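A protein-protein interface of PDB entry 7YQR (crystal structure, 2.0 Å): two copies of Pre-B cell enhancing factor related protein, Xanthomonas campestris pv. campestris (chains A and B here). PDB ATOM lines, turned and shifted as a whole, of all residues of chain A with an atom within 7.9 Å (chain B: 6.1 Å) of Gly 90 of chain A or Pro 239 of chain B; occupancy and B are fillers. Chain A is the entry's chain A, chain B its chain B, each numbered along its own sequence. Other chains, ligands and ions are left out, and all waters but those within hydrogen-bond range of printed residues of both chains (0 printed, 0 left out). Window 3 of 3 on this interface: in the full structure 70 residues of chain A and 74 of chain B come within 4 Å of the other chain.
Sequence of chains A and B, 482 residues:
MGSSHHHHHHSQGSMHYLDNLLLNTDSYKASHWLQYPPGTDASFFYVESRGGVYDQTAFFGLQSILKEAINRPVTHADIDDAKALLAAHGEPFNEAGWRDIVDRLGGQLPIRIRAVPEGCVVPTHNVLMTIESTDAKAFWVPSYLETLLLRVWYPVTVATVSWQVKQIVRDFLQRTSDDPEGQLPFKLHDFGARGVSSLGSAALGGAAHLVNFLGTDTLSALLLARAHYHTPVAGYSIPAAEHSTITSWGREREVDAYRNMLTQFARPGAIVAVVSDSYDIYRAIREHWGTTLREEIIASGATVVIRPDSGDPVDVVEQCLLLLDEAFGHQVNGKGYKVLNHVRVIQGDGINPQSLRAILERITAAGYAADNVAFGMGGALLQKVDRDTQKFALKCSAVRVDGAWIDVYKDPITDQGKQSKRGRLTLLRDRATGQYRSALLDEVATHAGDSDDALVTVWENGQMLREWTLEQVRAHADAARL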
ATOM      1  N   SER A  27      12.208  19.586 -15.505  1.00  0.00           N
ATOM      2  CA  SER A  27      13.030  18.415 -15.186  1.00  0.00           C
ATOM      3  C   SER A  27      12.971  18.067 -13.709  1.00  0.00           C
ATOM      4  O   SER A  27      12.772  16.902 -13.345  1.00  0.00           O
ATOM      5  CB  SER A  27      14.492  18.644 -15.598  1.00  0.00           C
ATOM      6  OG  SER A  27      14.589  19.111 -16.931  1.00  0.00           O
ATOM      7  N   TYR A  28      13.169  19.060 -12.841  1.00  0.00           N
ATOM      8  CA  TYR A  28      13.338  18.745 -11.429  1.00  0.00           C
ATOM      9  C   TYR A  28      12.068  18.175 -10.799  1.00  0.00           C
ATOM     10  O   TYR A  28      12.142  17.550  -9.733  1.00  0.00           O
ATOM     11  CB  TYR A  28      13.801  19.978 -10.663  1.00  0.00           C
ATOM     12  CG  TYR A  28      12.736  21.023 -10.451  1.00  0.00           C
ATOM     13  CD1 TYR A  28      12.445  21.953 -11.439  1.00  0.00           C
ATOM     14  CD2 TYR A  28      12.020  21.082  -9.259  1.00  0.00           C
ATOM     15  CE1 TYR A  28      11.467  22.915 -11.249  1.00  0.00           C
ATOM     16  CE2 TYR A  28      11.044  22.033  -9.059  1.00  0.00           C
ATOM     17  CZ  TYR A  28      10.768  22.949 -10.056  1.00  0.00           C
ATOM     18  OH  TYR A  28       9.792  23.906  -9.868  1.00  0.00           O
ATOM     19  N   LYS A  29      10.910  18.358 -11.443  1.00  0.00           N
ATOM     20  CA  LYS A  29       9.665  17.806 -10.917  1.00  0.00           C
ATOM     21  C   LYS A  29       9.598  16.292 -11.071  1.00  0.00           C
ATOM     22  O   LYS A  29       8.812  15.636 -10.373  1.00  0.00           O
ATOM     23  CB  LYS A  29       8.473  18.481 -11.612  1.00  0.00           C
ATOM     24  CG  LYS A  29       7.935  19.639 -10.785  1.00  0.00           C
ATOM     25  CD  LYS A  29       7.050  20.522 -11.601  1.00  0.00           C
ATOM     26  CE  LYS A  29       6.006  19.678 -12.257  1.00  0.00           C
ATOM     27  NZ  LYS A  29       5.398  20.202 -13.501  1.00  0.00           N
ATOM     28  N   ALA A  30      10.383  15.728 -11.991  1.00  0.00           N
ATOM     29  CA  ALA A  30      10.412  14.279 -12.140  1.00  0.00           C
ATOM     30  C   ALA A  30      10.912  13.604 -10.868  1.00  0.00           C
ATOM     31  O   ALA A  30      10.450  12.512 -10.512  1.00  0.00           O
ATOM     32  CB  ALA A  30      11.291  13.886 -13.330  1.00  0.00           C
ATOM     33  N   SER A  31      11.861  14.237 -10.176  1.00  0.00           N
ATOM     34  CA  SER A  31      12.423  13.709  -8.941  1.00  0.00           C
ATOM     35  C   SER A  31      11.548  13.985  -7.729  1.00  0.00           C
ATOM     36  O   SER A  31      11.821  13.446  -6.647  1.00  0.00           O
ATOM     37  CB  SER A  31      13.812  14.313  -8.704  1.00  0.00           C
ATOM     38  OG  SER A  31      13.695  15.618  -8.143  1.00  0.00           O
ATOM     39  N   HIS A  32      10.491  14.775  -7.897  1.00  0.00           N
ATOM     40  CA  HIS A  32       9.801  15.374  -6.759  1.00  0.00           C
ATOM     41  C   HIS A  32       9.208  14.342  -5.806  1.00  0.00           C
ATOM     42  O   HIS A  32       9.197  14.556  -4.588  1.00  0.00           O
ATOM     43  CB  HIS A  32       8.704  16.299  -7.262  1.00  0.00           C
ATOM     44  CG  HIS A  32       8.428  17.440  -6.347  1.00  0.00           C
ATOM     45  ND1 HIS A  32       9.048  18.664  -6.485  1.00  0.00           N
ATOM     46  CD2 HIS A  32       7.619  17.541  -5.267  1.00  0.00           C
ATOM     47  CE1 HIS A  32       8.616  19.476  -5.538  1.00  0.00           C
ATOM     48  NE2 HIS A  32       7.751  18.820  -4.784  1.00  0.00           N
ATOM     49  N   LEU A  34      10.181  11.779  -4.548  1.00  0.00           N
ATOM     50  CA  LEU A  34      11.109  11.323  -3.522  1.00  0.00           C
ATOM     51  C   LEU A  34      11.238  12.287  -2.354  1.00  0.00           C
ATOM     52  O   LEU A  34      11.888  11.947  -1.362  1.00  0.00           O
ATOM     53  CB  LEU A  34      12.492  11.103  -4.133  1.00  0.00           C
ATOM     54  CG  LEU A  34      12.555  10.059  -5.241  1.00  0.00           C
ATOM     55  CD1 LEU A  34      13.831  10.247  -6.041  1.00  0.00           C
ATOM     56  CD2 LEU A  34      12.483   8.668  -4.633  1.00  0.00           C
ATOM     57  N   GLN A  35      10.656  13.477  -2.445  1.00  0.00           N
ATOM     58  CA  GLN A  35      10.892  14.515  -1.457  1.00  0.00           C
ATOM     59  C   GLN A  35       9.780  14.625  -0.424  1.00  0.00           C
ATOM     60  O   GLN A  35       9.919  15.392   0.533  1.00  0.00           O
ATOM     61  CB  GLN A  35      11.108  15.859  -2.164  1.00  0.00           C
ATOM     62  CG  GLN A  35      12.265  15.810  -3.167  1.00  0.00           C
ATOM     63  CD  GLN A  35      12.656  17.176  -3.701  1.00  0.00           C
ATOM     64  OE1 GLN A  35      12.581  18.180  -2.992  1.00  0.00           O
ATOM     65  NE2 GLN A  35      13.082  17.218  -4.961  1.00  0.00           N
ATOM     66  N   ALA A  84      14.087   6.664 -20.650  1.00  0.00           N
ATOM     67  CA  ALA A  84      15.357   6.763 -21.362  1.00  0.00           C
ATOM     68  C   ALA A  84      15.856   8.204 -21.408  1.00  0.00           C
ATOM     69  O   ALA A  84      17.035   8.480 -21.146  1.00  0.00           O
ATOM     70  CB  ALA A  84      15.196   6.198 -22.772  1.00  0.00           C
ATOM     71  N   LEU A  85      14.967   9.145 -21.729  1.00  0.00           N
ATOM     72  CA  LEU A  85      15.400  10.530 -21.866  1.00  0.00           C
ATOM     73  C   LEU A  85      15.825  11.108 -20.525  1.00  0.00           C
ATOM     74  O   LEU A  85      16.859  11.779 -20.430  1.00  0.00           O
ATOM     75  CB  LEU A  85      14.293  11.380 -22.493  1.00  0.00           C
ATOM     76  CG  LEU A  85      14.689  12.841 -22.703  1.00  0.00           C
ATOM     77  CD1 LEU A  85      15.897  12.940 -23.627  1.00  0.00           C
ATOM     78  CD2 LEU A  85      13.529  13.636 -23.255  1.00  0.00           C
ATOM     79  N   LEU A  86      15.050  10.854 -19.470  1.00  0.00           N
ATOM     80  CA  LEU A  86      15.360  11.485 -18.190  1.00  0.00           C
ATOM     81  C   LEU A  86      16.649  10.923 -17.590  1.00  0.00           C
ATOM     82  O   LEU A  86      17.408  11.656 -16.943  1.00  0.00           O
ATOM     83  CB  LEU A  86      14.192  11.321 -17.221  1.00  0.00           C
ATOM     84  CG  LEU A  86      12.994  12.243 -17.549  1.00  0.00           C
ATOM     85  CD1 LEU A  86      11.732  11.802 -16.791  1.00  0.00           C
ATOM     86  CD2 LEU A  86      13.323  13.683 -17.238  1.00  0.00           C
ATOM     87  N   ALA A  87      16.917   9.633 -17.802  1.00  0.00           N
ATOM     88  CA  ALA A  87      18.173   9.071 -17.313  1.00  0.00           C
ATOM     89  C   ALA A  87      19.365   9.645 -18.074  1.00  0.00           C
ATOM     90  O   ALA A  87      20.401   9.944 -17.475  1.00  0.00           O
ATOM     91  CB  ALA A  87      18.140   7.548 -17.409  1.00  0.00           C
ATOM     92  N   ALA A  88      19.238   9.832 -19.387  1.00  0.00           N
ATOM     93  CA  ALA A  88      20.331  10.459 -20.131  1.00  0.00           C
ATOM     94  C   ALA A  88      20.478  11.939 -19.779  1.00  0.00           C
ATOM     95  O   ALA A  88      21.594  12.474 -19.790  1.00  0.00           O
ATOM     96  CB  ALA A  88      20.104  10.296 -21.632  1.00  0.00           C
ATOM     97  N   HIS A  89      19.366  12.607 -19.449  1.00  0.00           N
ATOM     98  CA  HIS A  89      19.359  14.037 -19.149  1.00  0.00           C
ATOM     99  C   HIS A  89      19.893  14.322 -17.747  1.00  0.00           C
ATOM    100  O   HIS A  89      20.480  15.386 -17.513  1.00  0.00           O
ATOM    101  CB  HIS A  89      17.921  14.553 -19.343  1.00  0.00           C
ATOM    102  CG  HIS A  89      17.661  15.951 -18.873  1.00  0.00           C
ATOM    103  ND1 HIS A  89      18.139  17.067 -19.532  1.00  0.00           N
ATOM    104  CD2 HIS A  89      16.875  16.418 -17.872  1.00  0.00           C
ATOM    105  CE1 HIS A  89      17.705  18.159 -18.925  1.00  0.00           C
ATOM    106  NE2 HIS A  89      16.929  17.794 -17.918  1.00  0.00           N
ATOM    107  N   GLY A  90      19.720  13.389 -16.812  1.00  0.00           N
ATOM    108  CA  GLY A  90      20.225  13.579 -15.463  1.00  0.00           C
ATOM    109  C   GLY A  90      19.208  13.561 -14.328  1.00  0.00           C
ATOM    110  O   GLY A  90      19.539  13.943 -13.200  1.00  0.00           O
ATOM    111  N   GLU A  91      17.970  13.136 -14.593  1.00  0.00           N
ATOM    112  CA  GLU A  91      16.956  13.200 -13.544  1.00  0.00           C
ATOM    113  C   GLU A  91      16.456  11.808 -13.190  1.00  0.00           C
ATOM    114  O   GLU A  91      16.328  10.955 -14.073  1.00  0.00           O
ATOM    115  CB  GLU A  91      15.742  14.056 -13.972  1.00  0.00           C
ATOM    116  CG  GLU A  91      16.052  15.511 -14.174  1.00  0.00           C
ATOM    117  CD  GLU A  91      16.007  16.319 -12.896  1.00  0.00           C
ATOM    118  OE1 GLU A  91      15.659  15.758 -11.828  1.00  0.00           O
ATOM    119  OE2 GLU A  91      16.312  17.529 -12.966  1.00  0.00           O
ATOM    120  N   PRO A  92      16.159  11.549 -11.920  1.00  0.00           N
ATOM    121  CA  PRO A  92      15.488  10.293 -11.569  1.00  0.00           C
ATOM    122  C   PRO A  92      14.052  10.306 -12.069  1.00  0.00           C
ATOM    123  O   PRO A  92      13.445  11.361 -12.258  1.00  0.00           O
ATOM    124  CB  PRO A  92      15.543  10.264 -10.036  1.00  0.00           C
ATOM    125  CG  PRO A  92      16.383  11.451  -9.621  1.00  0.00           C
ATOM    126  CD  PRO A  92      16.372  12.422 -10.757  1.00  0.00           C
ATOM    127  N   PHE A  93      13.510   9.111 -12.281  1.00  0.00           N
ATOM    128  CA  PHE A  93      12.201   8.944 -12.894  1.00  0.00           C
ATOM    129  C   PHE A  93      11.460   7.821 -12.182  1.00  0.00           C
ATOM    130  O   PHE A  93      12.014   6.739 -11.991  1.00  0.00           O
ATOM    131  CB  PHE A  93      12.337   8.630 -14.384  1.00  0.00           C
ATOM    132  CG  PHE A  93      11.035   8.302 -15.066  1.00  0.00           C
ATOM    133  CD1 PHE A  93      10.034   9.247 -15.156  1.00  0.00           C
ATOM    134  CD2 PHE A  93      10.828   7.050 -15.632  1.00  0.00           C
ATOM    135  CE1 PHE A  93       8.838   8.958 -15.791  1.00  0.00           C
ATOM    136  CE2 PHE A  93       9.636   6.747 -16.266  1.00  0.00           C
ATOM    137  CZ  PHE A  93       8.640   7.707 -16.346  1.00  0.00           C
ATOM    138  N   TYR B 236      21.153  19.081 -20.199  1.00  0.00           N
ATOM    139  CA  TYR B 236      21.263  18.280 -18.980  1.00  0.00           C
ATOM    140  C   TYR B 236      20.757  19.060 -17.776  1.00  0.00           C
ATOM    141  O   TYR B 236      20.710  20.285 -17.784  1.00  0.00           O
ATOM    142  CB  TYR B 236      22.721  17.874 -18.712  1.00  0.00           C
ATOM    143  CG  TYR B 236      23.365  17.125 -19.855  1.00  0.00           C
ATOM    144  CD1 TYR B 236      23.021  15.809 -20.119  1.00  0.00           C
ATOM    145  CD2 TYR B 236      24.316  17.734 -20.664  1.00  0.00           C
ATOM    146  CE1 TYR B 236      23.594  15.111 -21.161  1.00  0.00           C
ATOM    147  CE2 TYR B 236      24.898  17.051 -21.719  1.00  0.00           C
ATOM    148  CZ  TYR B 236      24.531  15.735 -21.962  1.00  0.00           C
ATOM    149  OH  TYR B 236      25.101  15.027 -22.997  1.00  0.00           O
ATOM    150  N   SER B 237      20.452  18.342 -16.697  1.00  0.00           N
ATOM    151  CA  SER B 237      20.187  19.017 -15.440  1.00  0.00           C
ATOM    152  C   SER B 237      20.574  18.071 -14.297  1.00  0.00           C
ATOM    153  O   SER B 237      21.139  16.991 -14.517  1.00  0.00           O
ATOM    154  CB  SER B 237      18.723  19.498 -15.420  1.00  0.00           C
ATOM    155  OG  SER B 237      18.336  19.984 -14.170  1.00  0.00           O
ATOM    156  N   ILE B 238      20.333  18.515 -13.066  1.00  0.00           N
ATOM    157  CA  ILE B 238      20.591  17.730 -11.858  1.00  0.00           C
ATOM    158  C   ILE B 238      19.392  17.857 -10.931  1.00  0.00           C
ATOM    159  O   ILE B 238      18.645  18.842 -10.997  1.00  0.00           O
ATOM    160  CB  ILE B 238      21.862  18.200 -11.127  1.00  0.00           C
ATOM    161  CG1 ILE B 238      21.726  19.680 -10.769  1.00  0.00           C
ATOM    162  CG2 ILE B 238      23.106  17.918 -11.958  1.00  0.00           C
ATOM    163  CD1 ILE B 238      22.962  20.281 -10.137  1.00  0.00           C
ATOM    164  N   PRO B 239      19.189  16.885 -10.041  1.00  0.00           N
ATOM    165  CA  PRO B 239      18.053  16.975  -9.113  1.00  0.00           C
ATOM    166  C   PRO B 239      18.236  18.097  -8.096  1.00  0.00           C
ATOM    167  O   PRO B 239      19.356  18.532  -7.804  1.00  0.00           O
ATOM    168  CB  PRO B 239      18.030  15.600  -8.438  1.00  0.00           C
ATOM    169  CG  PRO B 239      19.420  15.085  -8.582  1.00  0.00           C
ATOM    170  CD  PRO B 239      19.910  15.607  -9.899  1.00  0.00           C
ATOM    171  N   ALA B 240      17.100  18.565  -7.562  1.00  0.00           N
ATOM    172  CA  ALA B 240      17.036  19.739  -6.691  1.00  0.00           C
ATOM    173  C   ALA B 240      15.814  19.671  -5.773  1.00  0.00           C
ATOM    174  O   ALA B 240      14.874  18.913  -6.022  1.00  0.00           O
ATOM    175  CB  ALA B 240      16.982  21.028  -7.515  1.00  0.00           C
ATOM    176  N   ALA B 241      15.819  20.512  -4.724  1.00  0.00           N
ATOM    177  CA  ALA B 241      14.741  20.609  -3.739  1.00  0.00           C
ATOM    178  C   ALA B 241      13.761  21.725  -4.133  1.00  0.00           C
ATOM    179  O   ALA B 241      13.798  22.245  -5.253  1.00  0.00           O
ATOM    180  CB  ALA B 241      15.320  20.817  -2.338  1.00  0.00           C
ATOM    181  N   MET B 261      17.765  14.021   0.761  1.00  0.00           N
ATOM    182  CA  MET B 261      18.239  13.868  -0.609  1.00  0.00           C
ATOM    183  C   MET B 261      19.765  13.806  -0.694  1.00  0.00           C
ATOM    184  O   MET B 261      20.306  13.591  -1.783  1.00  0.00           O
ATOM    185  CB  MET B 261      17.682  14.998  -1.498  1.00  0.00           C
ATOM    186  CG  MET B 261      17.861  14.764  -3.025  1.00  0.00           C
ATOM    187  SD  MET B 261      16.397  14.288  -3.990  1.00  0.00           S
ATOM    188  CE  MET B 261      17.155  13.787  -5.532  1.00  0.00           C
ATOM    189  N   ILE B 271      26.408  15.534  -8.316  1.00  0.00           N
ATOM    190  CA  ILE B 271      26.037  16.905  -7.980  1.00  0.00           C
ATOM    191  C   ILE B 271      24.532  17.010  -7.712  1.00  0.00           C
ATOM    192  O   ILE B 271      23.735  16.346  -8.373  1.00  0.00           O
ATOM    193  CB  ILE B 271      26.458  17.875  -9.100  1.00  0.00           C
ATOM    194  CG1 ILE B 271      27.879  17.557  -9.573  1.00  0.00           C
ATOM    195  CG2 ILE B 271      26.359  19.318  -8.630  1.00  0.00           C
ATOM    196  CD1 ILE B 271      28.531  18.675 -10.355  1.00  0.00           C
ATOM    197  N   VAL B 272      24.147  17.836  -6.733  1.00  0.00           N
ATOM    198  CA  VAL B 272      22.751  18.043  -6.356  1.00  0.00           C
ATOM    199  C   VAL B 272      22.557  19.500  -5.949  1.00  0.00           C
ATOM    200  O   VAL B 272      23.494  20.185  -5.535  1.00  0.00           O
ATOM    201  CB  VAL B 272      22.319  17.122  -5.197  1.00  0.00           C
ATOM    202  CG1 VAL B 272      22.335  15.658  -5.623  1.00  0.00           C
ATOM    203  CG2 VAL B 272      23.224  17.352  -3.997  1.00  0.00           C
ATOM    204  N   ALA B 273      21.322  19.977  -6.068  1.00  0.00           N
ATOM    205  CA  ALA B 273      20.992  21.368  -5.777  1.00  0.00           C
ATOM    206  C   ALA B 273      20.084  21.463  -4.555  1.00  0.00           C
ATOM    207  O   ALA B 273      19.010  20.850  -4.526  1.00  0.00           O
ATOM    208  CB  ALA B 273      20.315  22.035  -6.976  1.00  0.00           C
ATOM    209  N   VAL B 274      20.501  22.247  -3.560  1.00  0.00           N
ATOM    210  CA  VAL B 274      19.714  22.489  -2.356  1.00  0.00           C
ATOM    211  C   VAL B 274      19.385  23.975  -2.282  1.00  0.00           C
ATOM    212  O   VAL B 274      20.213  24.824  -2.630  1.00  0.00           O
ATOM    213  CB  VAL B 274      20.450  22.008  -1.085  1.00  0.00           C
ATOM    214  CG1 VAL B 274      20.946  20.582  -1.267  1.00  0.00           C
ATOM    215  CG2 VAL B 274      21.606  22.922  -0.736  1.00  0.00           C
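O of Ala 240 of chain B is in hydrogen-bond range of NE2 of Gln 35 of chain A. The backbone carbonyl oxygen (O) of His 89 of chain A sits at hydrogen-bond distance from the backbone NH (N) of Ser 237 of chain B, at 3.1 Å. The side-chain hydroxyl (OG) of Ser 237 of chain B sits at hydrogen-bond distance from the side-chain carboxylate (OE2) of Glu 91 of chain A (3.4 Å). The side-chain carboxylate of Glu 91 of chain A sits close to the backbone carbonyl oxygen of Ile 238 of chain B (3.3 Å).
The side-chain hydroxyl of Ser 27 of chain A is in hydrogen-bond range of a ring nitrogen (NE2) of His 89 of chain A (2.9 Å). The side-chain carboxylate (OE2) of Glu 91 of chain A lies within hydrogen-bond range of the backbone NH (N) of Tyr 28 of chain A, at 3.5 Å. The backbone NH (N) of Glu 91 of chain A lies within hydrogen-bond range of the backbone carbonyl oxygen (O) of Leu 86 of chain A, 2.8 Å away. The backbone NH (N) of Ala 273 of chain B sits at hydrogen-bond distance from the backbone carbonyl oxygen (O) of Pro 239 of chain B. The backbone carbonyl oxygen (O) of Ala 273 of chain B is in hydrogen-bond range of the backbone NH (N) of Ala 241 of chain B, at 3.2 Å.
Gln 35 of chain A touches Ala 241 of chain B. CE1 of Tyr 236 of chain B touches O of Ala 88 of chain A (3.6 Å). CA of Tyr 236 of chain B touches O of His 89 of chain A, 3.3 Å away. Gly 90 of chain A touches Ser 237 of chain B. Gly 90 of chain A touches Pro 239 of chain B (O to CD, 3.7 Å). Glu 91 of chain A touches Pro 239 of chain B (OE1 to CA, 3.8 Å).
Of the printed residues of chain B, Ala 88 of chain A touches Tyr 236. Of chain B, only Ser 237 and Pro 239 come within 4 Å of Gly 90 of chain A. Pro 92 of chain A touches none of the printed residues of chain B. Printed residues of chain A within 4 Å of Tyr 236 of chain B: Ala 88 (3.6 Å) and His 89 (3.3 Å). Val 272 of chain B touches none of the printed residues of chain A. The nearest residue of chain A that does not touch Pro 239 of chain B is Pro 92 of chain A (4.3 Å). The nearest printed residue of chain A that does not touch Ala 241 of chain B is Tyr 28 of chain A (4.5 Å).
Of the 18 printed residues of chain A, 5 touch a printed residue of chain B. Along chain A the printed residues that touch a printed residue of chain B span positions 35 to 91. Printed residues of chain B that touch a printed residue of chain A: Tyr 236, Ser 237, Ile 238, Pro 239, Ala 240 and Ala 241. Among the printed residues, no Asp or Glu carboxylate lies within 4 Å of a Lys or Arg side-chain nitrogen of the other chain.
No position is printed for both chains. Of the 10 pairs that touch across the chains among the printed residues, none has its exchanged pair printed and touching as well.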
